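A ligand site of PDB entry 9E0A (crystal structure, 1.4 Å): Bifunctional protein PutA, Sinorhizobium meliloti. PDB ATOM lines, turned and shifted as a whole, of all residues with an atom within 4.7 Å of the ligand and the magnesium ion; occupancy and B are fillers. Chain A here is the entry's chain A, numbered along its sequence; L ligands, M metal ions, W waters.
The magnesium ion is bound by water W2 (2.0 Å), an oxygen (O2) of the ligand (2.1 Å), water W10 (2.1 Å), water W7 (2.1 Å), water W4 (2.1 Å) and water W1 (2.2 Å). The magnesium ion has six donor atoms within binding distance.
The backbone carbonyl oxygen of Gly 784 lies close to an oxygen (O11) of the ligand, 3.4 Å away. Merely in contact with the ligand: Pro 707 (3.1 Å), Asn 709 (3.2 Å), Ile 705 (3.2 Å), Phe 1012 (3.2 Å), Phe 782 (3.2 Å), Ile 714 (3.3 Å), Thr 783 (3.3 Å), Gly 814 (3.3 Å), Val 788 (3.4 Å), Glu 812 (3.4 Å), Ala 769 (3.4 Å), Phe 944 (3.5 Å), Gly 768 (3.5 Å), Gly 765 (3.5 Å), Ile 792 (3.7 Å), Asp 764 (3.7 Å), Phe 710 (3.8 Å), Pro 733 (3.8 Å), Ser 1018 (3.9 Å), Leu 791 (3.9 Å) and Leu 972 (3.96 Å). The nearest printed residue that does not touch the ligand is Gln 795 (4.1 Å).
O1 of the ligand sits at hydrogen-bond distance from N of Ser 785 (2.8 Å). OG of Ser 785 lies within hydrogen-bond range of O1 of the ligand (2.6 Å). O6 of the ligand lies within hydrogen-bond range of OE1 of Glu 735, at 2.6 Å. OE1 of Glu 942 lies within hydrogen-bond range of O12 of the ligand. The side-chain amino group (NZ) of Lys 732 lies within hydrogen-bond range of an oxygen (O6) of the ligand. O of Ser 706 is in hydrogen-bond range of O5 of the ligand (2.7 Å). N7 of the ligand sits at hydrogen-bond distance from O of Thr 813 (2.8 Å). SG of Cys 846 lies close to O14 of the ligand (3.7 Å). N of Trp 708 lies within hydrogen-bond range of O9 of the ligand, at 2.9 Å. The backbone NH (N) of Ala 734 lies close to an oxygen (O5) of the ligand (3.5 Å).
No residue comes within 4 Å of the magnesium ion. The nearest printed residue that does not touch the magnesium ion is Glu 735 (4.3 Å).
The side-chain hydroxyl (OG) of Ser 785 sits close to the backbone NH (N) of Val 788, 3.3 Å away. N of Ser 706 lies within hydrogen-bond range of O of Lys 732, at 3.4 Å. NZ of Lys 732 sits at hydrogen-bond distance from O of Gly 763, at 2.7 Å. The backbone NH (N) of Ala 734 sits at hydrogen-bond distance from the backbone carbonyl oxygen (O) of Ser 706, at 3.3 Å. The backbone NH of Thr 813 is in hydrogen-bond range of the backbone carbonyl oxygen of Ser 1018 (2.9 Å). The backbone carbonyl oxygen of Glu 812 sits at hydrogen-bond distance from the backbone NH of Gly 784 (3.0 Å). The backbone NH (N) of Thr 783 is in hydrogen-bond range of the backbone carbonyl oxygen (O) of Ile 705, 3.0 Å away. N of Glu 812 lies within hydrogen-bond range of O of Phe 782, 2.9 Å away.
Water W7 lies within hydrogen-bond range of O8 of the ligand (2.7 Å) and OE2 of Glu 736 (2.9 Å). Water W4 bridges OE2 of Glu 735 (2.7 Å) and O3 of the ligand (3.3 Å). Water W5 lies within hydrogen-bond range of an oxygen (O9) of the ligand (2.6 Å) and the side-chain carboxylate of Glu 736 (2.8 Å). Water W8 lies within hydrogen-bond range of OE1 of Glu 812 (2.7 Å), O of Ser 1018 (2.7 Å) and N7 of the ligand (3.1 Å). Water W3 bridges the side-chain carboxylate (OE1) of Glu 942 (2.9 Å) and an oxygen (O12) of the ligand (3.4 Å).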
ATOM      1  N   ILE A 705      20.183  21.656 -26.616  1.00  0.00           N
ATOM      2  CA  ILE A 705      20.130  20.215 -26.760  1.00  0.00           C
ATOM      3  C   ILE A 705      20.144  19.635 -25.353  1.00  0.00           C
ATOM      4  O   ILE A 705      21.021  19.956 -24.547  1.00  0.00           O
ATOM      5  CB  ILE A 705      21.326  19.709 -27.597  1.00  0.00           C
ATOM      6  CG1 ILE A 705      21.213  20.192 -29.043  1.00  0.00           C
ATOM      7  CG2 ILE A 705      21.405  18.206 -27.556  1.00  0.00           C
ATOM      8  CD1 ILE A 705      22.516  20.056 -29.789  1.00  0.00           C
ATOM      9  N   SER A 706      19.152  18.803 -25.059  1.00  0.00           N
ATOM     10  CA  SER A 706      18.899  18.393 -23.686  1.00  0.00           C
ATOM     11  C   SER A 706      18.879  16.872 -23.576  1.00  0.00           C
ATOM     12  O   SER A 706      18.634  16.171 -24.555  1.00  0.00           O
ATOM     13  CB  SER A 706      17.584  18.988 -23.176  1.00  0.00           C
ATOM     14  OG  SER A 706      16.528  18.727 -24.085  1.00  0.00           O
ATOM     15  N   PRO A 707      19.108  16.356 -22.378  1.00  0.00           N
ATOM     16  CA  PRO A 707      19.146  14.900 -22.175  1.00  0.00           C
ATOM     17  C   PRO A 707      17.767  14.357 -21.834  1.00  0.00           C
ATOM     18  O   PRO A 707      16.838  15.098 -21.505  1.00  0.00           O
ATOM     19  CB  PRO A 707      20.055  14.782 -20.945  1.00  0.00           C
ATOM     20  CG  PRO A 707      19.708  15.980 -20.154  1.00  0.00           C
ATOM     21  CD  PRO A 707      19.513  17.083 -21.168  1.00  0.00           C
ATOM     22  N   TRP A 708      17.642  13.034 -21.926  1.00  0.00           N
ATOM     23  CA  TRP A 708      16.343  12.448 -21.653  1.00  0.00           C
ATOM     24  C   TRP A 708      16.013  12.406 -20.172  1.00  0.00           C
ATOM     25  O   TRP A 708      14.829  12.378 -19.812  1.00  0.00           O
ATOM     26  CB  TRP A 708      16.255  11.022 -22.245  1.00  0.00           C
ATOM     27  CG  TRP A 708      17.015  10.033 -21.412  1.00  0.00           C
ATOM     28  CD1 TRP A 708      18.287   9.609 -21.629  1.00  0.00           C
ATOM     29  CD2 TRP A 708      16.560   9.378 -20.226  1.00  0.00           C
ATOM     30  NE1 TRP A 708      18.670   8.732 -20.632  1.00  0.00           N
ATOM     31  CE2 TRP A 708      17.626   8.581 -19.759  1.00  0.00           C
ATOM     32  CE3 TRP A 708      15.360   9.389 -19.500  1.00  0.00           C
ATOM     33  CZ2 TRP A 708      17.526   7.801 -18.609  1.00  0.00           C
ATOM     34  CZ3 TRP A 708      15.264   8.626 -18.352  1.00  0.00           C
ATOM     35  CH2 TRP A 708      16.343   7.834 -17.917  1.00  0.00           C
ATOM     36  N   ASN A 709      17.016  12.436 -19.296  1.00  0.00           N
ATOM     37  CA  ASN A 709      16.802  11.957 -17.931  1.00  0.00           C
ATOM     38  C   ASN A 709      16.180  13.003 -17.013  1.00  0.00           C
ATOM     39  O   ASN A 709      15.594  12.628 -15.990  1.00  0.00           O
ATOM     40  CB  ASN A 709      18.099  11.438 -17.336  1.00  0.00           C
ATOM     41  CG  ASN A 709      19.057  12.545 -17.029  1.00  0.00           C
ATOM     42  OD1 ASN A 709      19.558  13.209 -17.936  1.00  0.00           O
ATOM     43  ND2 ASN A 709      19.306  12.762 -15.745  1.00  0.00           N
ATOM     44  N   PHE A 710      16.339  14.279 -17.320  1.00  0.00           N
ATOM     45  CA  PHE A 710      15.604  15.355 -16.667  1.00  0.00           C
ATOM     46  C   PHE A 710      14.843  16.038 -17.796  1.00  0.00           C
ATOM     47  O   PHE A 710      15.192  17.147 -18.220  1.00  0.00           O
ATOM     48  CB  PHE A 710      16.538  16.329 -15.962  1.00  0.00           C
ATOM     49  CG  PHE A 710      17.334  15.722 -14.832  1.00  0.00           C
ATOM     50  CD1 PHE A 710      16.758  14.794 -13.974  1.00  0.00           C
ATOM     51  CD2 PHE A 710      18.664  16.077 -14.634  1.00  0.00           C
ATOM     52  CE1 PHE A 710      17.485  14.249 -12.939  1.00  0.00           C
ATOM     53  CE2 PHE A 710      19.397  15.519 -13.599  1.00  0.00           C
ATOM     54  CZ  PHE A 710      18.811  14.610 -12.749  1.00  0.00           C
ATOM     55  N   ILE A 714      15.815  20.239 -17.170  1.00  0.00           N
ATOM     56  CA  ILE A 714      16.977  20.735 -17.894  1.00  0.00           C
ATOM     57  C   ILE A 714      16.557  21.321 -19.225  1.00  0.00           C
ATOM     58  O   ILE A 714      17.078  22.357 -19.665  1.00  0.00           O
ATOM     59  CB  ILE A 714      18.041  19.633 -18.047  1.00  0.00           C
ATOM     60  CG1 ILE A 714      18.619  19.331 -16.656  1.00  0.00           C
ATOM     61  CG2 ILE A 714      19.121  20.033 -19.087  1.00  0.00           C
ATOM     62  CD1 ILE A 714      19.975  18.732 -16.669  1.00  0.00           C
ATOM     63  N   LYS A 732      15.969  21.178 -29.070  1.00  0.00           N
ATOM     64  CA  LYS A 732      16.110  19.806 -29.563  1.00  0.00           C
ATOM     65  C   LYS A 732      16.090  18.892 -28.356  1.00  0.00           C
ATOM     66  O   LYS A 732      17.133  18.649 -27.729  1.00  0.00           O
ATOM     67  CB  LYS A 732      17.423  19.658 -30.339  1.00  0.00           C
ATOM     68  CG  LYS A 732      17.347  18.710 -31.534  1.00  0.00           C
ATOM     69  CD  LYS A 732      16.951  17.296 -31.109  1.00  0.00           C
ATOM     70  CE  LYS A 732      18.095  16.607 -30.370  1.00  0.00           C
ATOM     71  NZ  LYS A 732      17.661  15.272 -29.859  1.00  0.00           N
ATOM     72  N   PRO A 733      14.940  18.348 -27.976  1.00  0.00           N
ATOM     73  CA  PRO A 733      14.899  17.454 -26.825  1.00  0.00           C
ATOM     74  C   PRO A 733      15.422  16.078 -27.197  1.00  0.00           C
ATOM     75  O   PRO A 733      15.479  15.694 -28.367  1.00  0.00           O
ATOM     76  CB  PRO A 733      13.404  17.377 -26.516  1.00  0.00           C
ATOM     77  CG  PRO A 733      12.754  17.534 -27.859  1.00  0.00           C
ATOM     78  CD  PRO A 733      13.613  18.539 -28.586  1.00  0.00           C
ATOM     79  N   ALA A 734      15.828  15.350 -26.161  1.00  0.00           N
ATOM     80  CA  ALA A 734      16.304  13.988 -26.368  1.00  0.00           C
ATOM     81  C   ALA A 734      15.246  13.169 -27.087  1.00  0.00           C
ATOM     82  O   ALA A 734      14.041  13.328 -26.872  1.00  0.00           O
ATOM     83  CB  ALA A 734      16.575  13.347 -25.014  1.00  0.00           C
ATOM     84  N   GLU A 735      15.703  12.254 -27.945  1.00  0.00           N
ATOM     85  CA  GLU A 735      14.767  11.455 -28.731  1.00  0.00           C
ATOM     86  C   GLU A 735      13.890  10.569 -27.854  1.00  0.00           C
ATOM     87  O   GLU A 735      12.809  10.153 -28.298  1.00  0.00           O
ATOM     88  CB  GLU A 735      15.507  10.619 -29.768  1.00  0.00           C
ATOM     89  CG  GLU A 735      16.582   9.697 -29.197  1.00  0.00           C
ATOM     90  CD  GLU A 735      17.964  10.349 -29.152  1.00  0.00           C
ATOM     91  OE1 GLU A 735      18.031  11.602 -29.059  1.00  0.00           O
ATOM     92  OE2 GLU A 735      18.970   9.616 -29.207  1.00  0.00           O
ATOM     93  N   GLU A 736      14.310  10.273 -26.623  1.00  0.00           N
ATOM     94  CA  GLU A 736      13.530   9.373 -25.784  1.00  0.00           C
ATOM     95  C   GLU A 736      12.335  10.084 -25.160  1.00  0.00           C
ATOM     96  O   GLU A 736      11.321   9.434 -24.873  1.00  0.00           O
ATOM     97  CB  GLU A 736      14.407   8.801 -24.671  1.00  0.00           C
ATOM     98  CG  GLU A 736      15.563   7.938 -25.158  1.00  0.00           C
ATOM     99  CD  GLU A 736      16.852   8.730 -25.326  1.00  0.00           C
ATOM    100  OE1 GLU A 736      16.798   9.973 -25.455  1.00  0.00           O
ATOM    101  OE2 GLU A 736      17.927   8.089 -25.344  1.00  0.00           O
ATOM    102  N   GLY A 763      13.643  14.860 -32.454  1.00  0.00           N
ATOM    103  CA  GLY A 763      14.450  13.980 -33.267  1.00  0.00           C
ATOM    104  C   GLY A 763      15.675  13.534 -32.501  1.00  0.00           C
ATOM    105  O   GLY A 763      15.851  13.840 -31.328  1.00  0.00           O
ATOM    106  N   ASP A 764      16.551  12.809 -33.197  1.00  0.00           N
ATOM    107  CA  ASP A 764      17.699  12.197 -32.553  1.00  0.00           C
ATOM    108  C   ASP A 764      18.940  13.100 -32.673  1.00  0.00           C
ATOM    109  O   ASP A 764      18.823  14.297 -32.931  1.00  0.00           O
ATOM    110  CB  ASP A 764      17.914  10.763 -33.082  1.00  0.00           C
ATOM    111  CG  ASP A 764      18.165  10.716 -34.591  1.00  0.00           C
ATOM    112  OD1 ASP A 764      18.640  11.714 -35.164  1.00  0.00           O
ATOM    113  OD2 ASP A 764      17.873   9.657 -35.205  1.00  0.00           O
ATOM    114  N   GLY A 765      20.124  12.517 -32.477  1.00  0.00           N
ATOM    115  CA  GLY A 765      21.349  13.283 -32.531  1.00  0.00           C
ATOM    116  C   GLY A 765      21.604  13.942 -33.870  1.00  0.00           C
ATOM    117  O   GLY A 765      22.283  14.975 -33.933  1.00  0.00           O
ATOM    118  N   GLY A 768      20.130  17.324 -33.623  1.00  0.00           N
ATOM    119  CA  GLY A 768      21.023  18.151 -32.832  1.00  0.00           C
ATOM    120  C   GLY A 768      22.240  18.592 -33.618  1.00  0.00           C
ATOM    121  O   GLY A 768      22.611  19.765 -33.605  1.00  0.00           O
ATOM    122  N   ALA A 769      22.856  17.656 -34.343  1.00  0.00           N
ATOM    123  CA  ALA A 769      24.072  17.967 -35.080  1.00  0.00           C
ATOM    124  C   ALA A 769      23.783  18.943 -36.218  1.00  0.00           C
ATOM    125  O   ALA A 769      24.583  19.848 -36.485  1.00  0.00           O
ATOM    126  CB  ALA A 769      24.707  16.689 -35.618  1.00  0.00           C
ATOM    127  N   PHE A 782      24.347  22.562 -24.332  1.00  0.00           N
ATOM    128  CA  PHE A 782      24.270  21.121 -24.377  1.00  0.00           C
ATOM    129  C   PHE A 782      24.308  20.566 -22.962  1.00  0.00           C
ATOM    130  O   PHE A 782      25.215  20.907 -22.186  1.00  0.00           O
ATOM    131  CB  PHE A 782      25.466  20.531 -25.127  1.00  0.00           C
ATOM    132  CG  PHE A 782      25.499  19.039 -25.122  1.00  0.00           C
ATOM    133  CD1 PHE A 782      24.663  18.320 -25.955  1.00  0.00           C
ATOM    134  CD2 PHE A 782      26.327  18.348 -24.264  1.00  0.00           C
ATOM    135  CE1 PHE A 782      24.659  16.942 -25.947  1.00  0.00           C
ATOM    136  CE2 PHE A 782      26.333  16.975 -24.258  1.00  0.00           C
ATOM    137  CZ  PHE A 782      25.502  16.265 -25.099  1.00  0.00           C
ATOM    138  N   THR A 783      23.373  19.690 -22.653  1.00  0.00           N
ATOM    139  CA  THR A 783      23.495  18.843 -21.470  1.00  0.00           C
ATOM    140  C   THR A 783      23.298  17.420 -21.943  1.00  0.00           C
ATOM    141  O   THR A 783      22.343  17.121 -22.657  1.00  0.00           O
ATOM    142  CB  THR A 783      22.481  19.248 -20.395  1.00  0.00           C
ATOM    143  OG1 THR A 783      22.692  20.621 -20.057  1.00  0.00           O
ATOM    144  CG2 THR A 783      22.692  18.410 -19.142  1.00  0.00           C
ATOM    145  N   GLY A 784      24.231  16.548 -21.576  1.00  0.00           N
ATOM    146  CA  GLY A 784      24.222  15.196 -22.110  1.00  0.00           C
ATOM    147  C   GLY A 784      25.528  14.514 -21.796  1.00  0.00           C
ATOM    148  O   GLY A 784      26.267  14.939 -20.912  1.00  0.00           O
ATOM    149  N   SER A 785      25.813  13.459 -22.547  1.00  0.00           N
ATOM    150  CA  SER A 785      27.015  12.686 -22.278  1.00  0.00           C
ATOM    151  C   SER A 785      28.270  13.427 -22.710  1.00  0.00           C
ATOM    152  O   SER A 785      28.257  14.248 -23.636  1.00  0.00           O
ATOM    153  CB  SER A 785      26.938  11.331 -22.988  1.00  0.00           C
ATOM    154  OG  SER A 785      26.940  11.503 -24.403  1.00  0.00           O
ATOM    155  N   VAL A 788      29.151  12.766 -26.426  1.00  0.00           N
ATOM    156  CA  VAL A 788      28.427  13.567 -27.406  1.00  0.00           C
ATOM    157  C   VAL A 788      28.908  15.011 -27.374  1.00  0.00           C
ATOM    158  O   VAL A 788      29.094  15.637 -28.430  1.00  0.00           O
ATOM    159  CB  VAL A 788      26.912  13.442 -27.182  1.00  0.00           C
ATOM    160  CG1 VAL A 788      26.174  14.470 -28.038  1.00  0.00           C
ATOM    161  CG2 VAL A 788      26.467  12.052 -27.558  1.00  0.00           C
ATOM    162  N   LEU A 791      31.765  15.407 -29.585  1.00  0.00           N
ATOM    163  CA  LEU A 791      31.404  15.524 -30.997  1.00  0.00           C
ATOM    164  C   LEU A 791      30.926  16.936 -31.328  1.00  0.00           C
ATOM    165  O   LEU A 791      31.308  17.500 -32.363  1.00  0.00           O
ATOM    166  CB  LEU A 791      30.312  14.514 -31.318  1.00  0.00           C
ATOM    167  CG  LEU A 791      30.689  13.032 -31.186  1.00  0.00           C
ATOM    168  CD1 LEU A 791      29.469  12.155 -31.382  1.00  0.00           C
ATOM    169  CD2 LEU A 791      31.771  12.666 -32.182  1.00  0.00           C
ATOM    170  N   ILE A 792      30.111  17.529 -30.450  1.00  0.00           N
ATOM    171  CA  ILE A 792      29.683  18.903 -30.671  1.00  0.00           C
ATOM    172  C   ILE A 792      30.870  19.855 -30.635  1.00  0.00           C
ATOM    173  O   ILE A 792      30.971  20.773 -31.460  1.00  0.00           O
ATOM    174  CB  ILE A 792      28.596  19.275 -29.638  1.00  0.00           C
ATOM    175  CG1 ILE A 792      27.342  18.481 -29.930  1.00  0.00           C
ATOM    176  CG2 ILE A 792      28.340  20.788 -29.657  1.00  0.00           C
ATOM    177  CD1 ILE A 792      26.331  18.541 -28.845  1.00  0.00           C
ATOM    178  N   GLN A 795      32.460  19.727 -33.969  1.00  0.00           N
ATOM    179  CA  GLN A 795      31.675  20.456 -34.961  1.00  0.00           C
ATOM    180  C   GLN A 795      31.916  21.953 -34.863  1.00  0.00           C
ATOM    181  O   GLN A 795      32.088  22.628 -35.886  1.00  0.00           O
ATOM    182  CB  GLN A 795      30.188  20.196 -34.722  1.00  0.00           C
ATOM    183  CG  GLN A 795      29.599  18.927 -35.271  1.00  0.00           C
ATOM    184  CD  GLN A 795      28.080  18.943 -35.154  1.00  0.00           C
ATOM    185  OE1 GLN A 795      27.525  18.737 -34.065  1.00  0.00           O
ATOM    186  NE2 GLN A 795      27.404  19.233 -36.246  1.00  0.00           N
ATOM    187  N   GLU A 812      27.389  20.587 -20.349  1.00  0.00           N
ATOM    188  CA  GLU A 812      27.254  20.065 -19.008  1.00  0.00           C
ATOM    189  C   GLU A 812      27.073  18.563 -19.145  1.00  0.00           C
ATOM    190  O   GLU A 812      26.096  18.111 -19.747  1.00  0.00           O
ATOM    191  CB  GLU A 812      26.058  20.730 -18.322  1.00  0.00           C
ATOM    192  CG  GLU A 812      26.280  22.234 -18.193  1.00  0.00           C
ATOM    193  CD  GLU A 812      27.584  22.559 -17.455  1.00  0.00           C
ATOM    194  OE1 GLU A 812      27.594  22.481 -16.209  1.00  0.00           O
ATOM    195  OE2 GLU A 812      28.602  22.879 -18.115  1.00  0.00           O
ATOM    196  N   THR A 813      28.044  17.803 -18.636  1.00  0.00           N
ATOM    197  CA  THR A 813      28.207  16.419 -19.053  1.00  0.00           C
ATOM    198  C   THR A 813      28.206  15.442 -17.879  1.00  0.00           C
ATOM    199  O   THR A 813      27.638  15.745 -16.829  1.00  0.00           O
ATOM    200  CB  THR A 813      29.419  16.278 -19.978  1.00  0.00           C
ATOM    201  OG1 THR A 813      30.566  16.917 -19.401  1.00  0.00           O
ATOM    202  CG2 THR A 813      29.108  16.972 -21.308  1.00  0.00           C
ATOM    203  N   GLY A 814      28.826  14.281 -18.044  1.00  0.00           N
ATOM    204  CA  GLY A 814      28.636  13.181 -17.121  1.00  0.00           C
ATOM    205  C   GLY A 814      29.431  13.308 -15.837  1.00  0.00           C
ATOM    206  O   GLY A 814      30.249  14.199 -15.630  1.00  0.00           O
ATOM    207  N   GLY A 815      29.174  12.363 -14.918  1.00  0.00           N
ATOM    208  CA  GLY A 815      29.843  12.336 -13.647  1.00  0.00           C
ATOM    209  C   GLY A 815      30.340  10.948 -13.336  1.00  0.00           C
ATOM    210  O   GLY A 815      29.901   9.965 -13.917  1.00  0.00           O
ATOM    211  N   CYS A 846      22.552  12.552 -13.542  1.00  0.00           N
ATOM    212  CA  CYS A 846      23.966  12.851 -13.736  1.00  0.00           C
ATOM    213  C   CYS A 846      24.679  12.959 -12.407  1.00  0.00           C
ATOM    214  O   CYS A 846      25.874  12.663 -12.319  1.00  0.00           O
ATOM    215  CB  CYS A 846      24.130  14.127 -14.541  1.00  0.00           C
ATOM    216  SG  CYS A 846      23.219  15.520 -13.880  1.00  0.00           S
ATOM    217  N   GLU A 942      31.474   6.733 -17.136  1.00  0.00           N
ATOM    218  CA  GLU A 942      30.187   6.798 -16.457  1.00  0.00           C
ATOM    219  C   GLU A 942      29.294   5.663 -16.924  1.00  0.00           C
ATOM    220  O   GLU A 942      29.139   5.426 -18.121  1.00  0.00           O
ATOM    221  CB  GLU A 942      29.520   8.121 -16.812  1.00  0.00           C
ATOM    222  CG  GLU A 942      28.121   8.313 -16.249  1.00  0.00           C
ATOM    223  CD  GLU A 942      27.457   9.556 -16.799  1.00  0.00           C
ATOM    224  OE1 GLU A 942      27.428   9.680 -18.038  1.00  0.00           O
ATOM    225  OE2 GLU A 942      27.019  10.416 -16.011  1.00  0.00           O
ATOM    226  N   PHE A 944      25.500   4.873 -16.674  1.00  0.00           N
ATOM    227  CA  PHE A 944      24.315   5.666 -16.356  1.00  0.00           C
ATOM    228  C   PHE A 944      23.147   4.728 -16.065  1.00  0.00           C
ATOM    229  O   PHE A 944      22.231   4.530 -16.861  1.00  0.00           O
ATOM    230  CB  PHE A 944      24.001   6.608 -17.522  1.00  0.00           C
ATOM    231  CG  PHE A 944      23.163   7.796 -17.128  1.00  0.00           C
ATOM    232  CD1 PHE A 944      23.672   8.783 -16.315  1.00  0.00           C
ATOM    233  CD2 PHE A 944      21.881   7.940 -17.619  1.00  0.00           C
ATOM    234  CE1 PHE A 944      22.895   9.881 -15.974  1.00  0.00           C
ATOM    235  CE2 PHE A 944      21.109   9.047 -17.286  1.00  0.00           C
ATOM    236  CZ  PHE A 944      21.618  10.011 -16.464  1.00  0.00           C
ATOM    237  N   LEU A 972      31.678  16.225 -10.937  1.00  0.00           N
ATOM    238  CA  LEU A 972      30.316  16.722 -10.892  1.00  0.00           C
ATOM    239  C   LEU A 972      29.827  16.804  -9.445  1.00  0.00           C
ATOM    240  O   LEU A 972      29.959  17.857  -8.818  1.00  0.00           O
ATOM    241  CB  LEU A 972      29.407  15.886 -11.780  1.00  0.00           C
ATOM    242  CG  LEU A 972      27.989  16.447 -11.976  1.00  0.00           C
ATOM    243  CD1 LEU A 972      28.025  17.913 -12.437  1.00  0.00           C
ATOM    244  CD2 LEU A 972      27.246  15.594 -12.999  1.00  0.00           C
ATOM    245  N   PHE A1012      24.201  24.165 -10.064  1.00  0.00           N
ATOM    246  CA  PHE A1012      24.590  22.803 -10.364  1.00  0.00           C
ATOM    247  C   PHE A1012      25.474  22.785 -11.596  1.00  0.00           C
ATOM    248  O   PHE A1012      25.143  23.393 -12.620  1.00  0.00           O
ATOM    249  CB  PHE A1012      23.377  21.912 -10.603  1.00  0.00           C
ATOM    250  CG  PHE A1012      23.748  20.476 -10.770  1.00  0.00           C
ATOM    251  CD1 PHE A1012      23.999  19.683  -9.658  1.00  0.00           C
ATOM    252  CD2 PHE A1012      23.922  19.924 -12.031  1.00  0.00           C
ATOM    253  CE1 PHE A1012      24.380  18.366  -9.801  1.00  0.00           C
ATOM    254  CE2 PHE A1012      24.301  18.607 -12.189  1.00  0.00           C
ATOM    255  CZ  PHE A1012      24.536  17.830 -11.068  1.00  0.00           C
ATOM    256  N   SER A1018      33.088  16.703 -16.610  1.00  0.00           N
ATOM    257  CA  SER A1018      31.702  16.913 -16.210  1.00  0.00           C
ATOM    258  C   SER A1018      31.115  18.229 -16.671  1.00  0.00           C
ATOM    259  O   SER A1018      29.902  18.414 -16.544  1.00  0.00           O
ATOM    260  CB  SER A1018      31.576  16.851 -14.690  1.00  0.00           C
ATOM    261  OG  SER A1018      31.936  15.569 -14.243  1.00  0.00           O
HETATM  262  P1  LIG L   1      23.105  11.953 -24.746  1.00  0.00           P
HETATM  263  O1  LIG L   1      24.565  12.412 -24.819  1.00  0.00           O
HETATM  264  O2  LIG L   1      22.800  10.599 -25.171  1.00  0.00           O
HETATM  265  O3  LIG L   1      22.098  12.785 -25.486  1.00  0.00           O
HETATM  266  C1  LIG L   1      21.934  14.137 -25.138  1.00  0.00           C
HETATM  267  C2  LIG L   1      21.339  14.983 -26.253  1.00  0.00           C
HETATM  268  O4  LIG L   1      22.300  15.149 -27.279  1.00  0.00           O
HETATM  269  C3  LIG L   1      20.087  14.437 -26.878  1.00  0.00           C
HETATM  270  O5  LIG L   1      19.184  15.445 -27.148  1.00  0.00           O
HETATM  271  C4  LIG L   1      20.594  13.797 -28.102  1.00  0.00           C
HETATM  272  O6  LIG L   1      19.617  13.676 -29.082  1.00  0.00           O
HETATM  273  C5  LIG L   1      21.645  14.761 -28.476  1.00  0.00           C
HETATM  274  N1  LIG L   1      22.650  14.241 -29.358  1.00  0.00           N
HETATM  275  C6  LIG L   1      23.099  12.931 -29.479  1.00  0.00           C
HETATM  276  N2  LIG L   1      24.078  12.883 -30.379  1.00  0.00           N
HETATM  277  C7  LIG L   1      24.317  14.167 -30.866  1.00  0.00           C
HETATM  278  C8  LIG L   1      25.183  14.717 -31.788  1.00  0.00           C
HETATM  279  N3  LIG L   1      26.121  13.896 -32.486  1.00  0.00           N
HETATM  280  N4  LIG L   1      25.142  16.033 -32.021  1.00  0.00           N
HETATM  281  C9  LIG L   1      24.285  16.864 -31.388  1.00  0.00           C
HETATM  282  N5  LIG L   1      23.405  16.362 -30.489  1.00  0.00           N
HETATM  283  C10 LIG L   1      23.413  15.040 -30.215  1.00  0.00           C
HETATM  284  O7  LIG L   1      22.615  11.950 -23.313  1.00  0.00           O
HETATM  285  P2  LIG L   1      21.283  11.443 -22.573  1.00  0.00           P
HETATM  286  O8  LIG L   1      21.350   9.958 -22.553  1.00  0.00           O
HETATM  287  O9  LIG L   1      20.030  12.020 -23.160  1.00  0.00           O
HETATM  288  O10 LIG L   1      21.438  11.986 -21.080  1.00  0.00           O
HETATM  289  C11 LIG L   1      22.304  11.328 -20.188  1.00  0.00           C
HETATM  290  C12 LIG L   1      23.648  12.027 -20.025  1.00  0.00           C
HETATM  291  O11 LIG L   1      23.484  13.385 -19.714  1.00  0.00           O
HETATM  292  C13 LIG L   1      24.476  11.394 -18.949  1.00  0.00           C
HETATM  293  O12 LIG L   1      25.766  11.220 -19.365  1.00  0.00           O
HETATM  294  C14 LIG L   1      24.390  12.379 -17.873  1.00  0.00           C
HETATM  295  O13 LIG L   1      25.439  12.322 -16.954  1.00  0.00           O
HETATM  296  C15 LIG L   1      24.334  13.647 -18.632  1.00  0.00           C
HETATM  297  N6  LIG L   1      23.742  14.686 -17.849  1.00  0.00           N
HETATM  298  C16 LIG L   1      24.534  15.742 -17.336  1.00  0.00           C
HETATM  299  C17 LIG L   1      23.908  16.720 -16.570  1.00  0.00           C
HETATM  300  C18 LIG L   1      24.649  17.863 -15.970  1.00  0.00           C
HETATM  301  O14 LIG L   1      24.042  18.769 -15.417  1.00  0.00           O
HETATM  302  N7  LIG L   1      26.067  17.859 -16.021  1.00  0.00           N
HETATM  303  C19 LIG L   1      22.513  16.653 -16.351  1.00  0.00           C
HETATM  304  C20 LIG L   1      21.730  15.572 -16.819  1.00  0.00           C
HETATM  305  C21 LIG L   1      22.361  14.611 -17.574  1.00  0.00           C
HETATM  306 MG    MG M   1      22.087   9.073 -26.345  1.00  0.00          MG
HETATM  307  O   HOH W   1      23.545   9.393 -27.904  1.00  0.00           O
HETATM  308  O   HOH W   2      23.451   7.850 -25.479  1.00  0.00           O
HETATM  309  O   HOH W   3      29.168  11.114 -19.909  1.00  0.00           O
HETATM  310  O   HOH W   4      20.793  10.445 -27.367  1.00  0.00           O
HETATM  311  O   HOH W   5      19.176  11.384 -25.568  1.00  0.00           O
HETATM  312  O   HOH W   6      23.084   8.299 -21.746  1.00  0.00           O
HETATM  313  O   HOH W   7      20.668   8.745 -24.829  1.00  0.00           O
HETATM  314  O   HOH W   8      28.116  20.031 -15.291  1.00  0.00           O
HETATM  315  O   HOH W   9      23.195  21.281 -15.507  1.00  0.00           O
HETATM  316  O   HOH W  10      21.275   7.513 -27.434  1.00  0.00           O
